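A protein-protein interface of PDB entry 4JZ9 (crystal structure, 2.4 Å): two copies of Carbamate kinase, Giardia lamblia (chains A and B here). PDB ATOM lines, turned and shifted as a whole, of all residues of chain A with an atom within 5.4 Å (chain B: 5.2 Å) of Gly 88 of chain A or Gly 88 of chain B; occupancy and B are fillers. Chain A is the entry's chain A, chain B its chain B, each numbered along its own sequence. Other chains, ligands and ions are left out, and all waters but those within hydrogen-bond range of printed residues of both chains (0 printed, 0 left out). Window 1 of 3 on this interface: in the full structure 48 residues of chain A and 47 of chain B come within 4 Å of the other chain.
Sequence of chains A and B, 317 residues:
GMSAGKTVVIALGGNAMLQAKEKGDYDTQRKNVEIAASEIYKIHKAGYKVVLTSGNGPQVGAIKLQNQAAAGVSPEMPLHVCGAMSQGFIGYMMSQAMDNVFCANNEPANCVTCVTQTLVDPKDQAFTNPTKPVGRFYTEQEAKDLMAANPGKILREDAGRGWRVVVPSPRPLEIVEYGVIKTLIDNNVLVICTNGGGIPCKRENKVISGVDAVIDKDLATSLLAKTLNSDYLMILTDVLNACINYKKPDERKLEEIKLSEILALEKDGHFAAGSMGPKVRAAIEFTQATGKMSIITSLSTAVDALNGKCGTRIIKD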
ATOM      1  N   GLY A  83       6.876  10.410   8.144  1.00  0.00           N
ATOM      2  CA  GLY A  83       7.800   9.978   7.113  1.00  0.00           C
ATOM      3  C   GLY A  83       8.698   8.823   7.563  1.00  0.00           C
ATOM      4  O   GLY A  83       8.803   7.787   6.878  1.00  0.00           O
ATOM      5  N   ALA A  84       9.330   8.993   8.726  1.00  0.00           N
ATOM      6  CA  ALA A  84      10.131   7.943   9.344  1.00  0.00           C
ATOM      7  C   ALA A  84       9.377   6.643   9.365  1.00  0.00           C
ATOM      8  O   ALA A  84       9.901   5.615   9.001  1.00  0.00           O
ATOM      9  CB  ALA A  84      10.548   8.332  10.763  1.00  0.00           C
ATOM     10  N   MET A  85       8.131   6.684   9.803  1.00  0.00           N
ATOM     11  CA  MET A  85       7.330   5.472   9.829  1.00  0.00           C
ATOM     12  C   MET A  85       7.077   4.947   8.427  1.00  0.00           C
ATOM     13  O   MET A  85       6.900   3.750   8.229  1.00  0.00           O
ATOM     14  CB  MET A  85       6.001   5.713  10.517  1.00  0.00           C
ATOM     15  CG  MET A  85       6.105   6.028  11.956  1.00  0.00           C
ATOM     16  SD  MET A  85       4.422   6.262  12.563  1.00  0.00           S
ATOM     17  CE  MET A  85       4.711   6.395  14.344  1.00  0.00           C
ATOM     18  N   SER A  86       7.052   5.839   7.453  1.00  0.00           N
ATOM     19  CA  SER A  86       6.672   5.421   6.126  1.00  0.00           C
ATOM     20  C   SER A  86       7.862   4.722   5.494  1.00  0.00           C
ATOM     21  O   SER A  86       7.691   3.812   4.694  1.00  0.00           O
ATOM     22  CB  SER A  86       6.218   6.615   5.283  1.00  0.00           C
ATOM     23  OG  SER A  86       7.314   7.392   4.835  1.00  0.00           O
ATOM     24  N   GLN A  87       9.066   5.153   5.861  1.00  0.00           N
ATOM     25  CA  GLN A  87      10.261   4.516   5.348  1.00  0.00           C
ATOM     26  C   GLN A  87      10.342   3.112   5.934  1.00  0.00           C
ATOM     27  O   GLN A  87      10.832   2.203   5.280  1.00  0.00           O
ATOM     28  CB  GLN A  87      11.517   5.284   5.730  1.00  0.00           C
ATOM     29  CG  GLN A  87      11.612   6.722   5.298  1.00  0.00           C
ATOM     30  CD  GLN A  87      13.028   7.282   5.522  1.00  0.00           C
ATOM     31  OE1 GLN A  87      13.819   6.716   6.289  1.00  0.00           O
ATOM     32  NE2 GLN A  87      13.360   8.375   4.830  1.00  0.00           N
ATOM     33  N   GLY A  88       9.880   2.956   7.177  1.00  0.00           N
ATOM     34  CA  GLY A  88       9.779   1.660   7.816  1.00  0.00           C
ATOM     35  C   GLY A  88       8.841   0.781   7.027  1.00  0.00           C
ATOM     36  O   GLY A  88       9.177  -0.353   6.716  1.00  0.00           O
ATOM     37  N   PHE A  89       7.667   1.310   6.685  1.00  0.00           N
ATOM     38  CA  PHE A  89       6.655   0.586   5.883  1.00  0.00           C
ATOM     39  C   PHE A  89       7.206   0.221   4.511  1.00  0.00           C
ATOM     40  O   PHE A  89       7.319  -0.951   4.143  1.00  0.00           O
ATOM     41  CB  PHE A  89       5.415   1.465   5.704  1.00  0.00           C
ATOM     42  CG  PHE A  89       4.273   0.813   4.927  1.00  0.00           C
ATOM     43  CD1 PHE A  89       4.150  -0.581   4.829  1.00  0.00           C
ATOM     44  CD2 PHE A  89       3.307   1.615   4.292  1.00  0.00           C
ATOM     45  CE1 PHE A  89       3.075  -1.171   4.132  1.00  0.00           C
ATOM     46  CE2 PHE A  89       2.230   1.038   3.569  1.00  0.00           C
ATOM     47  CZ  PHE A  89       2.110  -0.349   3.490  1.00  0.00           C
ATOM     48  N   ILE A  90       7.543   1.258   3.757  1.00  0.00           N
ATOM     49  CA  ILE A  90       7.956   1.098   2.386  1.00  0.00           C
ATOM     50  C   ILE A  90       9.257   0.332   2.272  1.00  0.00           C
ATOM     51  O   ILE A  90       9.421  -0.496   1.383  1.00  0.00           O
ATOM     52  CB  ILE A  90       8.101   2.459   1.663  1.00  0.00           C
ATOM     53  CG1 ILE A  90       6.768   3.220   1.688  1.00  0.00           C
ATOM     54  CG2 ILE A  90       8.644   2.237   0.213  1.00  0.00           C
ATOM     55  CD1 ILE A  90       6.881   4.719   1.395  1.00  0.00           C
ATOM     56  N   GLY A  91      10.202   0.636   3.145  1.00  0.00           N
ATOM     57  CA  GLY A  91      11.466  -0.080   3.124  1.00  0.00           C
ATOM     58  C   GLY A  91      11.250  -1.572   3.349  1.00  0.00           C
ATOM     59  O   GLY A  91      11.787  -2.397   2.643  1.00  0.00           O
ATOM     60  N   TYR A  92      10.463  -1.918   4.343  1.00  0.00           N
ATOM     61  CA  TYR A  92      10.170  -3.312   4.587  1.00  0.00           C
ATOM     62  C   TYR A  92       9.604  -4.052   3.376  1.00  0.00           C
ATOM     63  O   TYR A  92       9.994  -5.185   3.090  1.00  0.00           O
ATOM     64  CB  TYR A  92       9.166  -3.387   5.714  1.00  0.00           C
ATOM     65  CG  TYR A  92       8.452  -4.705   5.898  1.00  0.00           C
ATOM     66  CD1 TYR A  92       9.149  -5.886   6.136  1.00  0.00           C
ATOM     67  CD2 TYR A  92       7.061  -4.741   5.937  1.00  0.00           C
ATOM     68  CE1 TYR A  92       8.461  -7.076   6.371  1.00  0.00           C
ATOM     69  CE2 TYR A  92       6.375  -5.896   6.180  1.00  0.00           C
ATOM     70  CZ  TYR A  92       7.057  -7.064   6.389  1.00  0.00           C
ATOM     71  OH  TYR A  92       6.307  -8.200   6.612  1.00  0.00           O
ATOM     72  N   MET A  93       8.667  -3.423   2.680  1.00  0.00           N
ATOM     73  CA  MET A  93       8.078  -4.028   1.497  1.00  0.00           C
ATOM     74  C   MET A  93       9.135  -4.308   0.428  1.00  0.00           C
ATOM     75  O   MET A  93       9.155  -5.378  -0.164  1.00  0.00           O
ATOM     76  CB  MET A  93       7.017  -3.092   0.919  1.00  0.00           C
ATOM     77  CG  MET A  93       5.683  -3.142   1.619  1.00  0.00           C
ATOM     78  SD  MET A  93       4.501  -2.006   0.830  1.00  0.00           S
ATOM     79  CE  MET A  93       3.053  -2.899   1.261  1.00  0.00           C
ATOM     80  N   VAL A 115      17.159   3.742   7.219  1.00  0.00           N
ATOM     81  CA  VAL A 115      16.427   4.935   7.590  1.00  0.00           C
ATOM     82  C   VAL A 115      17.258   6.158   7.182  1.00  0.00           C
ATOM     83  O   VAL A 115      18.454   6.222   7.402  1.00  0.00           O
ATOM     84  CB  VAL A 115      16.007   4.902   9.112  1.00  0.00           C
ATOM     85  CG1 VAL A 115      15.255   6.182   9.535  1.00  0.00           C
ATOM     86  CG2 VAL A 115      15.144   3.660   9.394  1.00  0.00           C
ATOM     87  N   GLY B  83       4.790  -3.078  12.970  1.00  0.00           N
ATOM     88  CA  GLY B  83       6.142  -3.374  13.388  1.00  0.00           C
ATOM     89  C   GLY B  83       7.152  -2.596  12.573  1.00  0.00           C
ATOM     90  O   GLY B  83       7.964  -1.817  13.114  1.00  0.00           O
ATOM     91  N   ALA B  84       7.093  -2.806  11.260  1.00  0.00           N
ATOM     92  CA  ALA B  84       7.949  -2.079  10.320  1.00  0.00           C
ATOM     93  C   ALA B  84       7.905  -0.570  10.587  1.00  0.00           C
ATOM     94  O   ALA B  84       8.955   0.087  10.674  1.00  0.00           O
ATOM     95  CB  ALA B  84       7.536  -2.388   8.879  1.00  0.00           C
ATOM     96  N   MET B  85       6.683  -0.037  10.723  1.00  0.00           N
ATOM     97  CA  MET B  85       6.480   1.376  11.043  1.00  0.00           C
ATOM     98  C   MET B  85       7.177   1.864  12.330  1.00  0.00           C
ATOM     99  O   MET B  85       7.751   2.976  12.385  1.00  0.00           O
ATOM    100  CB  MET B  85       4.975   1.685  11.101  1.00  0.00           C
ATOM    101  CG  MET B  85       4.369   2.114   9.760  1.00  0.00           C
ATOM    102  SD  MET B  85       2.553   2.081   9.687  1.00  0.00           S
ATOM    103  CE  MET B  85       2.309   2.830   8.076  1.00  0.00           C
ATOM    104  N   SER B  86       7.098   1.036  13.369  1.00  0.00           N
ATOM    105  CA  SER B  86       7.723   1.344  14.646  1.00  0.00           C
ATOM    106  C   SER B  86       9.253   1.349  14.520  1.00  0.00           C
ATOM    107  O   SER B  86       9.940   2.103  15.236  1.00  0.00           O
ATOM    108  CB  SER B  86       7.283   0.334  15.713  1.00  0.00           C
ATOM    109  OG  SER B  86       7.695  -0.979  15.360  1.00  0.00           O
ATOM    110  N   GLN B  87       9.786   0.511  13.623  1.00  0.00           N
ATOM    111  CA  GLN B  87      11.234   0.518  13.383  1.00  0.00           C
ATOM    112  C   GLN B  87      11.615   1.844  12.729  1.00  0.00           C
ATOM    113  O   GLN B  87      12.625   2.452  13.073  1.00  0.00           O
ATOM    114  CB  GLN B  87      11.693  -0.645  12.493  1.00  0.00           C
ATOM    115  CG  GLN B  87      11.489  -2.061  13.038  1.00  0.00           C
ATOM    116  CD  GLN B  87      12.182  -3.117  12.146  1.00  0.00           C
ATOM    117  OE1 GLN B  87      12.579  -2.807  11.026  1.00  0.00           O
ATOM    118  NE2 GLN B  87      12.325  -4.355  12.642  1.00  0.00           N
ATOM    119  N   GLY B  88      10.808   2.262  11.762  1.00  0.00           N
ATOM    120  CA  GLY B  88      11.017   3.517  11.075  1.00  0.00           C
ATOM    121  C   GLY B  88      11.155   4.615  12.101  1.00  0.00           C
ATOM    122  O   GLY B  88      12.156   5.321  12.077  1.00  0.00           O
ATOM    123  N   PHE B  89      10.150   4.731  12.989  1.00  0.00           N
ATOM    124  CA  PHE B  89      10.095   5.715  14.092  1.00  0.00           C
ATOM    125  C   PHE B  89      11.250   5.646  15.137  1.00  0.00           C
ATOM    126  O   PHE B  89      11.943   6.637  15.383  1.00  0.00           O
ATOM    127  CB  PHE B  89       8.741   5.568  14.790  1.00  0.00           C
ATOM    128  CG  PHE B  89       8.534   6.468  15.977  1.00  0.00           C
ATOM    129  CD1 PHE B  89       8.947   7.792  15.963  1.00  0.00           C
ATOM    130  CD2 PHE B  89       7.882   5.990  17.105  1.00  0.00           C
ATOM    131  CE1 PHE B  89       8.738   8.621  17.085  1.00  0.00           C
ATOM    132  CE2 PHE B  89       7.654   6.807  18.214  1.00  0.00           C
ATOM    133  CZ  PHE B  89       8.072   8.124  18.209  1.00  0.00           C
ATOM    134  N   ILE B  90      11.438   4.473  15.745  1.00  0.00           N
ATOM    135  CA  ILE B  90      12.448   4.286  16.776  1.00  0.00           C
ATOM    136  C   ILE B  90      13.863   4.472  16.193  1.00  0.00           C
ATOM    137  O   ILE B  90      14.680   5.225  16.722  1.00  0.00           O
ATOM    138  CB  ILE B  90      12.329   2.885  17.476  1.00  0.00           C
ATOM    139  CG1 ILE B  90      10.982   2.714  18.209  1.00  0.00           C
ATOM    140  CG2 ILE B  90      13.518   2.652  18.453  1.00  0.00           C
ATOM    141  CD1 ILE B  90      10.603   1.237  18.548  1.00  0.00           C
ATOM    142  N   GLY B  91      14.129   3.803  15.082  1.00  0.00           N
ATOM    143  CA  GLY B  91      15.384   3.981  14.369  1.00  0.00           C
ATOM    144  C   GLY B  91      15.697   5.432  14.044  1.00  0.00           C
ATOM    145  O   GLY B  91      16.846   5.888  14.102  1.00  0.00           O
ATOM    146  N   TYR B  92      14.657   6.174  13.711  1.00  0.00           N
ATOM    147  CA  TYR B  92      14.837   7.582  13.434  1.00  0.00           C
ATOM    148  C   TYR B  92      15.265   8.353  14.689  1.00  0.00           C
ATOM    149  O   TYR B  92      16.203   9.136  14.627  1.00  0.00           O
ATOM    150  CB  TYR B  92      13.562   8.159  12.854  1.00  0.00           C
ATOM    151  CG  TYR B  92      13.494   9.663  12.865  1.00  0.00           C
ATOM    152  CD1 TYR B  92      14.530  10.445  12.322  1.00  0.00           C
ATOM    153  CD2 TYR B  92      12.388  10.309  13.369  1.00  0.00           C
ATOM    154  CE1 TYR B  92      14.447  11.830  12.292  1.00  0.00           C
ATOM    155  CE2 TYR B  92      12.292  11.688  13.327  1.00  0.00           C
ATOM    156  CZ  TYR B  92      13.314  12.439  12.797  1.00  0.00           C
ATOM    157  OH  TYR B  92      13.195  13.804  12.800  1.00  0.00           O
ATOM    158  N   VAL B 115      16.184  -1.548   8.704  1.00  0.00           N
ATOM    159  CA  VAL B 115      14.936  -2.280   8.821  1.00  0.00           C
ATOM    160  C   VAL B 115      15.315  -3.739   8.881  1.00  0.00           C
ATOM    161  O   VAL B 115      16.183  -4.191   8.150  1.00  0.00           O
ATOM    162  CB  VAL B 115      14.006  -1.989   7.596  1.00  0.00           C
ATOM    163  CG1 VAL B 115      12.688  -2.764   7.668  1.00  0.00           C
ATOM    164  CG2 VAL B 115      13.733  -0.499   7.498  1.00  0.00           C
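Among the printed residues, pairs that only touch across the chains: Ala 84 of chain A with Gly 88 of chain B, Gly 88 of chain A with Ala 84 of chain B, Met 85 of chain A with Met 85 of chain B, Ala 84 of chain A with Tyr 92 of chain B, Tyr 92 of chain A with Ala 84 of chain B, Met 85 of chain A with Phe 89 of chain B and Gly 88 of chain A with Gly 88 of chain B.
Of the 12 printed residues of chain A, 4 touch a printed residue of chain B.
Printed residues of chain A that touch a printed residue of chain B: Ala 84, Met 85, Gly 88 and Tyr 92.
Among the printed residues, no Asp or Glu carboxylate lies within 4 Å of a Lys or Arg side-chain nitrogen of the other chain.
Ala 84 of chain A touches Gly 88 of chain B, and with the chains exchanged Gly 88 of chain A touches Ala 84 of chain B.
Ala 84 of chain A touches Tyr 92 of chain B, and with the chains exchanged Tyr 92 of chain A touches Ala 84 of chain B.
Met 85 of chain A touches its own counterpart, Met 85 of chain B.
Gly 88 of chain B touches its own counterpart, Gly 88 of chain A.
Positions printed for both chains: 83, 84, 85, 86, 87, 88, 89, 90, 91, 92 and 115.
Of the 7 pairs that touch across the chains among the printed residues, 6 have their exchanged pair printed and touching as well.
Gly 88 of chain B touches just these residues of chain A: Ala 84 and Gly 88.
Of the printed residues of chain B, Tyr 92 of chain A touches Ala 84.
Of the printed residues of chain B, Ala 84 of chain A touches Gly 88 and Tyr 92.
Of the printed residues of chain A, Tyr 92 of chain B touches Ala 84.
Gln 87 of chain B touches none of the printed residues of chain A.
Val 115 of chain B touches none of the printed residues of chain A.
The nearest printed residue of chain B that does not touch Gly 88 of chain A is Met 85 of chain B (4.4 Å).
The nearest residue of chain A that does not touch Gly 88 of chain B is Val 115 of chain A (4.1 Å).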
